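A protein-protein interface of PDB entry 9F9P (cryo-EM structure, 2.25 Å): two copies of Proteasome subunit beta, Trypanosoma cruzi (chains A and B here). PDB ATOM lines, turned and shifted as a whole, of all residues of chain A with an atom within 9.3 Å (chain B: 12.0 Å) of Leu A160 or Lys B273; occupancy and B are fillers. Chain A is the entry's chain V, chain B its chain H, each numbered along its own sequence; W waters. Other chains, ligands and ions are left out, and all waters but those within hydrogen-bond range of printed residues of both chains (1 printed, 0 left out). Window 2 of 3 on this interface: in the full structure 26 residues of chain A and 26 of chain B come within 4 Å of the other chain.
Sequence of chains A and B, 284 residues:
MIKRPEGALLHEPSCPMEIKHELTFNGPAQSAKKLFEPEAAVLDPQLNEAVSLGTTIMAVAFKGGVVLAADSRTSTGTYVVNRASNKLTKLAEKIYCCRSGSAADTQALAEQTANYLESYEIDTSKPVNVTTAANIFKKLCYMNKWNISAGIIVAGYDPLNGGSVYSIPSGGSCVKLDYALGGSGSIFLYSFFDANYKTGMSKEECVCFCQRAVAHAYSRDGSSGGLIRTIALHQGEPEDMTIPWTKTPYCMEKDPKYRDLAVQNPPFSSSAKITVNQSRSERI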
ATOM      1  N   LYS A 126      -1.076  -3.749  -3.409  1.00  0.00           N
ATOM      2  CA  LYS A 126      -1.276  -5.075  -2.833  1.00  0.00           C
ATOM      3  C   LYS A 126      -2.262  -5.873  -3.679  1.00  0.00           C
ATOM      4  O   LYS A 126      -3.045  -5.308  -4.428  1.00  0.00           O
ATOM      5  CB  LYS A 126      -1.866  -4.967  -1.428  1.00  0.00           C
ATOM      6  CG  LYS A 126      -0.865  -4.651  -0.329  1.00  0.00           C
ATOM      7  CD  LYS A 126      -1.485  -4.782   1.041  1.00  0.00           C
ATOM      8  CE  LYS A 126      -1.793  -6.221   1.417  1.00  0.00           C
ATOM      9  NZ  LYS A 126      -2.679  -6.307   2.602  1.00  0.00           N
ATOM     10  N   PRO A 127      -2.271  -7.221  -3.599  1.00  0.00           N
ATOM     11  CA  PRO A 127      -3.267  -8.013  -4.329  1.00  0.00           C
ATOM     12  C   PRO A 127      -4.616  -7.991  -3.617  1.00  0.00           C
ATOM     13  O   PRO A 127      -4.679  -7.930  -2.394  1.00  0.00           O
ATOM     14  CB  PRO A 127      -2.577  -9.378  -4.441  1.00  0.00           C
ATOM     15  CG  PRO A 127      -1.734  -9.459  -3.174  1.00  0.00           C
ATOM     16  CD  PRO A 127      -1.269  -8.044  -2.901  1.00  0.00           C
ATOM     17  N   VAL A 128      -5.690  -8.005  -4.408  1.00  0.00           N
ATOM     18  CA  VAL A 128      -7.034  -7.773  -3.901  1.00  0.00           C
ATOM     19  C   VAL A 128      -7.630  -9.053  -3.314  1.00  0.00           C
ATOM     20  O   VAL A 128      -7.332 -10.161  -3.750  1.00  0.00           O
ATOM     21  CB  VAL A 128      -7.951  -7.213  -5.002  1.00  0.00           C
ATOM     22  CG1 VAL A 128      -7.387  -5.967  -5.620  1.00  0.00           C
ATOM     23  CG2 VAL A 128      -8.177  -8.192  -6.113  1.00  0.00           C
ATOM     24  N   ASN A 129      -8.557  -8.845  -2.398  1.00  0.00           N
ATOM     25  CA  ASN A 129      -9.335  -9.872  -1.743  1.00  0.00           C
ATOM     26  C   ASN A 129     -10.610 -10.194  -2.516  1.00  0.00           C
ATOM     27  O   ASN A 129     -11.188  -9.333  -3.187  1.00  0.00           O
ATOM     28  CB  ASN A 129      -9.761  -9.438  -0.340  1.00  0.00           C
ATOM     29  CG  ASN A 129      -8.563  -9.150   0.551  1.00  0.00           C
ATOM     30  OD1 ASN A 129      -7.550  -9.842   0.508  1.00  0.00           O
ATOM     31  ND2 ASN A 129      -8.677  -8.105   1.354  1.00  0.00           N
ATOM     32  N   VAL A 130     -11.077 -11.439  -2.329  1.00  0.00           N
ATOM     33  CA  VAL A 130     -12.227 -11.949  -3.044  1.00  0.00           C
ATOM     34  C   VAL A 130     -13.457 -11.135  -2.678  1.00  0.00           C
ATOM     35  O   VAL A 130     -14.277 -10.844  -3.541  1.00  0.00           O
ATOM     36  CB  VAL A 130     -12.404 -13.459  -2.829  1.00  0.00           C
ATOM     37  CG1 VAL A 130     -13.547 -14.043  -3.644  1.00  0.00           C
ATOM     38  CG2 VAL A 130     -11.129 -14.207  -3.189  1.00  0.00           C
ATOM     39  N   THR A 131     -13.548 -10.704  -1.425  1.00  0.00           N
ATOM     40  CA  THR A 131     -14.733  -9.971  -0.969  1.00  0.00           C
ATOM     41  C   THR A 131     -14.877  -8.636  -1.708  1.00  0.00           C
ATOM     42  O   THR A 131     -15.968  -8.285  -2.113  1.00  0.00           O
ATOM     43  CB  THR A 131     -14.732  -9.843   0.558  1.00  0.00           C
ATOM     44  OG1 THR A 131     -15.938  -9.217   0.984  1.00  0.00           O
ATOM     45  CG2 THR A 131     -13.652  -8.922   1.067  1.00  0.00           C
ATOM     46  N   THR A 132     -13.789  -7.958  -2.037  1.00  0.00           N
ATOM     47  CA  THR A 132     -13.842  -6.733  -2.826  1.00  0.00           C
ATOM     48  C   THR A 132     -14.370  -6.993  -4.240  1.00  0.00           C
ATOM     49  O   THR A 132     -15.161  -6.194  -4.758  1.00  0.00           O
ATOM     50  CB  THR A 132     -12.461  -6.051  -2.862  1.00  0.00           C
ATOM     51  OG1 THR A 132     -12.099  -5.554  -1.567  1.00  0.00           O
ATOM     52  CG2 THR A 132     -12.392  -4.875  -3.806  1.00  0.00           C
ATOM     53  N   TYR A 157      -8.912 -17.048  -4.387  1.00  0.00           N
ATOM     54  CA  TYR A 157      -8.035 -17.241  -3.257  1.00  0.00           C
ATOM     55  C   TYR A 157      -7.406 -15.910  -2.889  1.00  0.00           C
ATOM     56  O   TYR A 157      -7.038 -15.151  -3.785  1.00  0.00           O
ATOM     57  CB  TYR A 157      -6.874 -18.157  -3.607  1.00  0.00           C
ATOM     58  CG  TYR A 157      -5.909 -18.371  -2.462  1.00  0.00           C
ATOM     59  CD1 TYR A 157      -6.235 -19.232  -1.415  1.00  0.00           C
ATOM     60  CD2 TYR A 157      -4.757 -17.608  -2.338  1.00  0.00           C
ATOM     61  CE1 TYR A 157      -5.379 -19.435  -0.350  1.00  0.00           C
ATOM     62  CE2 TYR A 157      -3.900 -17.766  -1.244  1.00  0.00           C
ATOM     63  CZ  TYR A 157      -4.218 -18.678  -0.255  1.00  0.00           C
ATOM     64  OH  TYR A 157      -3.383 -18.849   0.827  1.00  0.00           O
ATOM     65  N   ASP A 158      -7.338 -15.606  -1.590  1.00  0.00           N
ATOM     66  CA  ASP A 158      -6.517 -14.523  -1.046  1.00  0.00           C
ATOM     67  C   ASP A 158      -5.962 -14.971   0.310  1.00  0.00           C
ATOM     68  O   ASP A 158      -6.527 -15.856   0.967  1.00  0.00           O
ATOM     69  CB  ASP A 158      -7.309 -13.223  -0.891  1.00  0.00           C
ATOM     70  CG  ASP A 158      -8.437 -13.239   0.162  1.00  0.00           C
ATOM     71  OD1 ASP A 158      -8.125 -13.438   1.388  1.00  0.00           O
ATOM     72  OD2 ASP A 158      -9.640 -12.989  -0.202  1.00  0.00           O
ATOM     73  N   PRO A 159      -4.810 -14.423   0.765  1.00  0.00           N
ATOM     74  CA  PRO A 159      -4.188 -14.902   2.011  1.00  0.00           C
ATOM     75  C   PRO A 159      -4.884 -14.535   3.325  1.00  0.00           C
ATOM     76  O   PRO A 159      -4.687 -15.205   4.325  1.00  0.00           O
ATOM     77  CB  PRO A 159      -2.746 -14.373   1.944  1.00  0.00           C
ATOM     78  CG  PRO A 159      -2.756 -13.248   0.902  1.00  0.00           C
ATOM     79  CD  PRO A 159      -3.998 -13.425   0.047  1.00  0.00           C
ATOM     80  N   LEU A 160      -5.789 -13.567   3.310  1.00  0.00           N
ATOM     81  CA  LEU A 160      -6.539 -13.194   4.498  1.00  0.00           C
ATOM     82  C   LEU A 160      -7.628 -14.222   4.823  1.00  0.00           C
ATOM     83  O   LEU A 160      -7.651 -14.777   5.916  1.00  0.00           O
ATOM     84  CB  LEU A 160      -7.122 -11.803   4.229  1.00  0.00           C
ATOM     85  CG  LEU A 160      -7.505 -10.941   5.434  1.00  0.00           C
ATOM     86  CD1 LEU A 160      -6.270 -10.604   6.266  1.00  0.00           C
ATOM     87  CD2 LEU A 160      -8.207  -9.655   4.966  1.00  0.00           C
ATOM     88  N   ASN A 161      -8.509 -14.521   3.863  1.00  0.00           N
ATOM     89  CA  ASN A 161      -9.585 -15.469   4.082  1.00  0.00           C
ATOM     90  C   ASN A 161      -9.401 -16.816   3.376  1.00  0.00           C
ATOM     91  O   ASN A 161     -10.307 -17.633   3.399  1.00  0.00           O
ATOM     92  CB  ASN A 161     -10.916 -14.880   3.593  1.00  0.00           C
ATOM     93  CG  ASN A 161     -11.538 -13.916   4.582  1.00  0.00           C
ATOM     94  OD1 ASN A 161     -12.004 -14.348   5.635  1.00  0.00           O
ATOM     95  ND2 ASN A 161     -11.578 -12.626   4.237  1.00  0.00           N
ATOM     96  N   GLY A 162      -8.304 -17.088   2.671  1.00  0.00           N
ATOM     97  CA  GLY A 162      -8.192 -18.395   2.016  1.00  0.00           C
ATOM     98  C   GLY A 162      -9.030 -18.501   0.736  1.00  0.00           C
ATOM     99  O   GLY A 162      -9.088 -17.553  -0.026  1.00  0.00           O
ATOM    100  N   GLY A 163      -9.678 -19.651   0.504  1.00  0.00           N
ATOM    101  CA  GLY A 163     -10.540 -19.865  -0.668  1.00  0.00           C
ATOM    102  C   GLY A 163     -11.968 -19.403  -0.397  1.00  0.00           C
ATOM    103  O   GLY A 163     -12.479 -19.758   0.631  1.00  0.00           O
ATOM    104  N   SER A 164     -12.585 -18.558  -1.211  1.00  0.00           N
ATOM    105  CA  SER A 164     -13.937 -18.101  -0.929  1.00  0.00           C
ATOM    106  C   SER A 164     -14.829 -18.184  -2.162  1.00  0.00           C
ATOM    107  O   SER A 164     -14.345 -17.971  -3.249  1.00  0.00           O
ATOM    108  CB  SER A 164     -13.934 -16.664  -0.498  1.00  0.00           C
ATOM    109  OG  SER A 164     -13.248 -16.412   0.726  1.00  0.00           O
ATOM    110  N   TYR A 166     -18.718 -16.813  -3.615  1.00  0.00           N
ATOM    111  CA  TYR A 166     -19.868 -15.954  -3.475  1.00  0.00           C
ATOM    112  C   TYR A 166     -20.827 -16.162  -4.631  1.00  0.00           C
ATOM    113  O   TYR A 166     -20.410 -16.237  -5.751  1.00  0.00           O
ATOM    114  CB  TYR A 166     -19.480 -14.466  -3.488  1.00  0.00           C
ATOM    115  CG  TYR A 166     -18.690 -14.004  -2.304  1.00  0.00           C
ATOM    116  CD1 TYR A 166     -17.331 -14.224  -2.214  1.00  0.00           C
ATOM    117  CD2 TYR A 166     -19.307 -13.379  -1.229  1.00  0.00           C
ATOM    118  CE1 TYR A 166     -16.589 -13.879  -1.072  1.00  0.00           C
ATOM    119  CE2 TYR A 166     -18.596 -12.990  -0.099  1.00  0.00           C
ATOM    120  CZ  TYR A 166     -17.230 -13.229  -0.018  1.00  0.00           C
ATOM    121  OH  TYR A 166     -16.525 -12.802   1.094  1.00  0.00           O
ATOM    122  N   LYS A 176     -22.480 -15.695   0.702  1.00  0.00           N
ATOM    123  CA  LYS A 176     -21.211 -16.368   0.881  1.00  0.00           C
ATOM    124  C   LYS A 176     -21.354 -17.824   1.331  1.00  0.00           C
ATOM    125  O   LYS A 176     -21.753 -18.087   2.458  1.00  0.00           O
ATOM    126  CB  LYS A 176     -20.403 -15.663   1.974  1.00  0.00           C
ATOM    127  CG  LYS A 176     -18.969 -16.162   2.125  1.00  0.00           C
ATOM    128  CD  LYS A 176     -18.152 -15.352   3.114  1.00  0.00           C
ATOM    129  CE  LYS A 176     -16.671 -15.680   3.076  1.00  0.00           C
ATOM    130  NZ  LYS A 176     -16.447 -17.127   3.328  1.00  0.00           N
ATOM    131  N   VAL B 263     -21.976 -16.929   6.694  1.00  0.00           N
ATOM    132  CA  VAL B 263     -21.637 -15.661   7.328  1.00  0.00           C
ATOM    133  C   VAL B 263     -22.148 -14.472   6.522  1.00  0.00           C
ATOM    134  O   VAL B 263     -21.413 -13.865   5.772  1.00  0.00           O
ATOM    135  CB  VAL B 263     -20.141 -15.555   7.653  1.00  0.00           C
ATOM    136  CG1 VAL B 263     -19.855 -14.230   8.358  1.00  0.00           C
ATOM    137  CG2 VAL B 263     -19.695 -16.728   8.525  1.00  0.00           C
ATOM    138  N   GLN B 264     -23.381 -14.069   6.779  1.00  0.00           N
ATOM    139  CA  GLN B 264     -23.981 -12.947   6.064  1.00  0.00           C
ATOM    140  C   GLN B 264     -23.944 -11.638   6.843  1.00  0.00           C
ATOM    141  O   GLN B 264     -24.012 -10.609   6.212  1.00  0.00           O
ATOM    142  CB  GLN B 264     -25.450 -13.244   5.747  1.00  0.00           C
ATOM    143  CG  GLN B 264     -25.593 -14.291   4.655  1.00  0.00           C
ATOM    144  CD  GLN B 264     -25.079 -13.849   3.311  1.00  0.00           C
ATOM    145  OE1 GLN B 264     -24.036 -14.281   2.831  1.00  0.00           O
ATOM    146  NE2 GLN B 264     -25.856 -12.999   2.671  1.00  0.00           N
ATOM    147  N   ASN B 265     -23.866 -11.699   8.181  1.00  0.00           N
ATOM    148  CA  ASN B 265     -24.025 -10.537   9.054  1.00  0.00           C
ATOM    149  C   ASN B 265     -22.815 -10.333   9.964  1.00  0.00           C
ATOM    150  O   ASN B 265     -22.940 -10.398  11.183  1.00  0.00           O
ATOM    151  CB  ASN B 265     -25.243 -10.721   9.975  1.00  0.00           C
ATOM    152  CG  ASN B 265     -26.520 -10.843   9.174  1.00  0.00           C
ATOM    153  OD1 ASN B 265     -26.710 -10.108   8.196  1.00  0.00           O
ATOM    154  ND2 ASN B 265     -27.361 -11.788   9.542  1.00  0.00           N
ATOM    155  N   PRO B 266     -21.612 -10.081   9.421  1.00  0.00           N
ATOM    156  CA  PRO B 266     -20.425  -9.918  10.264  1.00  0.00           C
ATOM    157  C   PRO B 266     -20.474  -8.613  11.051  1.00  0.00           C
ATOM    158  O   PRO B 266     -20.951  -7.607  10.533  1.00  0.00           O
ATOM    159  CB  PRO B 266     -19.260  -9.875   9.258  1.00  0.00           C
ATOM    160  CG  PRO B 266     -19.876  -9.417   7.944  1.00  0.00           C
ATOM    161  CD  PRO B 266     -21.336  -9.836   7.990  1.00  0.00           C
ATOM    162  N   PRO B 267     -19.935  -8.577  12.281  1.00  0.00           N
ATOM    163  CA  PRO B 267     -19.917  -7.348  13.089  1.00  0.00           C
ATOM    164  C   PRO B 267     -19.025  -6.265  12.490  1.00  0.00           C
ATOM    165  O   PRO B 267     -18.117  -6.557  11.709  1.00  0.00           O
ATOM    166  CB  PRO B 267     -19.345  -7.805  14.451  1.00  0.00           C
ATOM    167  CG  PRO B 267     -18.495  -9.016  14.104  1.00  0.00           C
ATOM    168  CD  PRO B 267     -19.157  -9.661  12.894  1.00  0.00           C
ATOM    169  N   PHE B 268     -19.296  -5.013  12.855  1.00  0.00           N
ATOM    170  CA  PHE B 268     -18.496  -3.858  12.440  1.00  0.00           C
ATOM    171  C   PHE B 268     -17.061  -3.983  12.968  1.00  0.00           C
ATOM    172  O   PHE B 268     -16.879  -4.201  14.162  1.00  0.00           O
ATOM    173  CB  PHE B 268     -19.197  -2.598  12.962  1.00  0.00           C
ATOM    174  CG  PHE B 268     -18.659  -1.275  12.502  1.00  0.00           C
ATOM    175  CD1 PHE B 268     -18.340  -1.053  11.169  1.00  0.00           C
ATOM    176  CD2 PHE B 268     -18.506  -0.233  13.407  1.00  0.00           C
ATOM    177  CE1 PHE B 268     -17.863   0.188  10.750  1.00  0.00           C
ATOM    178  CE2 PHE B 268     -18.057   1.014  12.984  1.00  0.00           C
ATOM    179  CZ  PHE B 268     -17.743   1.225  11.659  1.00  0.00           C
ATOM    180  N   SER B 269     -16.040  -3.928  12.093  1.00  0.00           N
ATOM    181  CA  SER B 269     -14.683  -4.245  12.546  1.00  0.00           C
ATOM    182  C   SER B 269     -13.606  -3.356  11.924  1.00  0.00           C
ATOM    183  O   SER B 269     -13.841  -2.669  10.931  1.00  0.00           O
ATOM    184  CB  SER B 269     -14.370  -5.730  12.310  1.00  0.00           C
ATOM    185  OG  SER B 269     -13.807  -5.970  11.046  1.00  0.00           O
ATOM    186  N   SER B 270     -12.387  -3.460  12.470  1.00  0.00           N
ATOM    187  CA  SER B 270     -11.212  -2.750  11.952  1.00  0.00           C
ATOM    188  C   SER B 270     -10.453  -3.575  10.912  1.00  0.00           C
ATOM    189  O   SER B 270      -9.388  -3.169  10.479  1.00  0.00           O
ATOM    190  CB  SER B 270     -10.279  -2.380  13.096  1.00  0.00           C
ATOM    191  OG  SER B 270     -10.954  -1.566  14.058  1.00  0.00           O
ATOM    192  N   SER B 271     -10.957  -4.761  10.554  1.00  0.00           N
ATOM    193  CA  SER B 271     -10.308  -5.599   9.565  1.00  0.00           C
ATOM    194  C   SER B 271     -11.300  -6.053   8.491  1.00  0.00           C
ATOM    195  O   SER B 271     -12.513  -6.015   8.684  1.00  0.00           O
ATOM    196  CB  SER B 271      -9.638  -6.795  10.220  1.00  0.00           C
ATOM    197  OG  SER B 271      -9.000  -7.617   9.238  1.00  0.00           O
ATOM    198  N   ALA B 272     -10.768  -6.535   7.358  1.00  0.00           N
ATOM    199  CA  ALA B 272     -11.594  -7.051   6.267  1.00  0.00           C
ATOM    200  C   ALA B 272     -11.753  -8.574   6.347  1.00  0.00           C
ATOM    201  O   ALA B 272     -12.458  -9.166   5.521  1.00  0.00           O
ATOM    202  CB  ALA B 272     -10.995  -6.643   4.946  1.00  0.00           C
ATOM    203  N   LYS B 273     -11.096  -9.185   7.332  1.00  0.00           N
ATOM    204  CA  LYS B 273     -11.255 -10.594   7.614  1.00  0.00           C
ATOM    205  C   LYS B 273     -12.698 -10.862   8.049  1.00  0.00           C
ATOM    206  O   LYS B 273     -13.263 -10.089   8.814  1.00  0.00           O
ATOM    207  CB  LYS B 273     -10.225 -11.005   8.670  1.00  0.00           C
ATOM    208  CG  LYS B 273     -10.302 -12.457   9.113  1.00  0.00           C
ATOM    209  CD  LYS B 273      -9.025 -12.959   9.758  1.00  0.00           C
ATOM    210  CE  LYS B 273      -8.961 -14.473   9.860  1.00  0.00           C
ATOM    211  NZ  LYS B 273      -9.047 -15.140   8.533  1.00  0.00           N
ATOM    212  N   ILE B 274     -13.274 -11.946   7.519  1.00  0.00           N
ATOM    213  CA  ILE B 274     -14.629 -12.405   7.795  1.00  0.00           C
ATOM    214  C   ILE B 274     -14.553 -13.650   8.673  1.00  0.00           C
ATOM    215  O   ILE B 274     -13.803 -14.577   8.384  1.00  0.00           O
ATOM    216  CB  ILE B 274     -15.378 -12.664   6.468  1.00  0.00           C
ATOM    217  CG1 ILE B 274     -15.652 -11.354   5.720  1.00  0.00           C
ATOM    218  CG2 ILE B 274     -16.661 -13.452   6.712  1.00  0.00           C
ATOM    219  CD1 ILE B 274     -16.293 -11.512   4.352  1.00  0.00           C
ATOM    220  N   THR B 275     -15.326 -13.675   9.754  1.00  0.00           N
ATOM    221  CA  THR B 275     -15.088 -14.634  10.829  1.00  0.00           C
ATOM    222  C   THR B 275     -16.408 -15.338  11.194  1.00  0.00           C
ATOM    223  O   THR B 275     -16.623 -16.484  10.818  1.00  0.00           O
ATOM    224  CB  THR B 275     -14.379 -13.910  11.992  1.00  0.00           C
ATOM    225  OG1 THR B 275     -13.335 -13.070  11.493  1.00  0.00           O
ATOM    226  CG2 THR B 275     -13.785 -14.859  13.010  1.00  0.00           C
ATOM    227  N   VAL B 276     -17.303 -14.612  11.876  1.00  0.00           N
ATOM    228  CA  VAL B 276     -18.529 -15.129  12.478  1.00  0.00           C
ATOM    229  C   VAL B 276     -19.650 -14.107  12.271  1.00  0.00           C
ATOM    230  O   VAL B 276     -19.368 -12.956  11.944  1.00  0.00           O
ATOM    231  CB  VAL B 276     -18.342 -15.418  13.986  1.00  0.00           C
ATOM    232  CG1 VAL B 276     -17.260 -16.470  14.219  1.00  0.00           C
ATOM    233  CG2 VAL B 276     -18.059 -14.147  14.810  1.00  0.00           C
ATOM    234  N   ASN B 277     -20.897 -14.549  12.479  1.00  0.00           N
ATOM    235  CA  ASN B 277     -22.067 -13.679  12.503  1.00  0.00           C
ATOM    236  C   ASN B 277     -22.180 -13.012  13.876  1.00  0.00           C
ATOM    237  O   ASN B 277     -21.924 -13.611  14.914  1.00  0.00           O
ATOM    238  CB  ASN B 277     -23.381 -14.432  12.225  1.00  0.00           C
ATOM    239  CG  ASN B 277     -23.601 -14.781  10.771  1.00  0.00           C
ATOM    240  OD1 ASN B 277     -23.740 -13.897   9.926  1.00  0.00           O
ATOM    241  ND2 ASN B 277     -23.622 -16.068  10.461  1.00  0.00           N
ATOM    242  N   GLN B 278     -22.623 -11.763  13.873  1.00  0.00           N
ATOM    243  CA  GLN B 278     -22.925 -11.064  15.109  1.00  0.00           C
ATOM    244  C   GLN B 278     -24.116 -11.734  15.806  1.00  0.00           C
ATOM    245  O   GLN B 278     -25.134 -12.029  15.196  1.00  0.00           O
ATOM    246  CB  GLN B 278     -23.214  -9.601  14.769  1.00  0.00           C
ATOM    247  CG  GLN B 278     -23.030  -8.653  15.953  1.00  0.00           C
ATOM    248  CD  GLN B 278     -23.421  -7.247  15.580  1.00  0.00           C
ATOM    249  OE1 GLN B 278     -23.602  -6.913  14.405  1.00  0.00           O
ATOM    250  NE2 GLN B 278     -23.612  -6.431  16.598  1.00  0.00           N
HETATM  251  O   HOH W   1     -20.527 -18.498   4.683  1.00  0.00           O
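Among the printed residues, merely in contact across the chains: Leu A160 with Ala B272, Asn A161 with Ala B272, Asn A161 with Lys B273 and Tyr A166 with Ile B274.
N of Lys A176 lies within hydrogen-bond range of OE1 of Gln B264.
The side-chain amide oxygen (OD1) of Asn A161 sits close to the backbone carbonyl oxygen (O) of Ile B274.
The side-chain amino group of Lys B273 is in hydrogen-bond range of the backbone carbonyl oxygen of Leu A160 (3.0 Å).
Of the printed residues of chain A, Lys B273 touches Leu A160 and Asn A161.
No residue of chain B comes within 4 Å of Asp A158.
No residue of chain B comes within 4 Å of Pro A159.
Of chain B, only Ala B272 (3.8 Å), Lys B273 (3.95 Å) and Ile B274 (3.3 Å) come within 4 Å of Asn A161.
No residue of chain B comes within 4 Å of Gly A162.
Of the printed residues of chain B, Tyr A166 touches Ile B274 (3.5 Å).
Printed residues of chain A within 4 Å of Gln B264: Lys A176.
Of the printed residues of chain B, Lys A176 touches Gln B264 (3.0 Å).
Asn A129 touches none of the printed residues of chain B.
Val A128 touches none of the printed residues of chain B.
Water W1 bridges O of Lys A176 and N of Val B263.
No position is printed for both chains.
The side-chain carboxylate of Asp A158 is in hydrogen-bond range of the backbone NH of Leu A160.
The backbone NH of Lys B273 is in hydrogen-bond range of the side-chain hydroxyl of Ser B271.
The backbone NH of Gln B264 sits at hydrogen-bond distance from the side-chain amide oxygen of Asn B277, 3.2 Å away.
OD1 of Asp A158 sits at hydrogen-bond distance from N of Asn A161 (2.7 Å).
Printed residues of chain B that touch a printed residue of chain A: Gln B264, Ala B272, Lys B273 and Ile B274.
Among the printed residues, 7 pairs touch across the chains.
Among the printed residues, no Asp or Glu carboxylate lies within 4 Å of a Lys or Arg side-chain nitrogen of the other chain.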
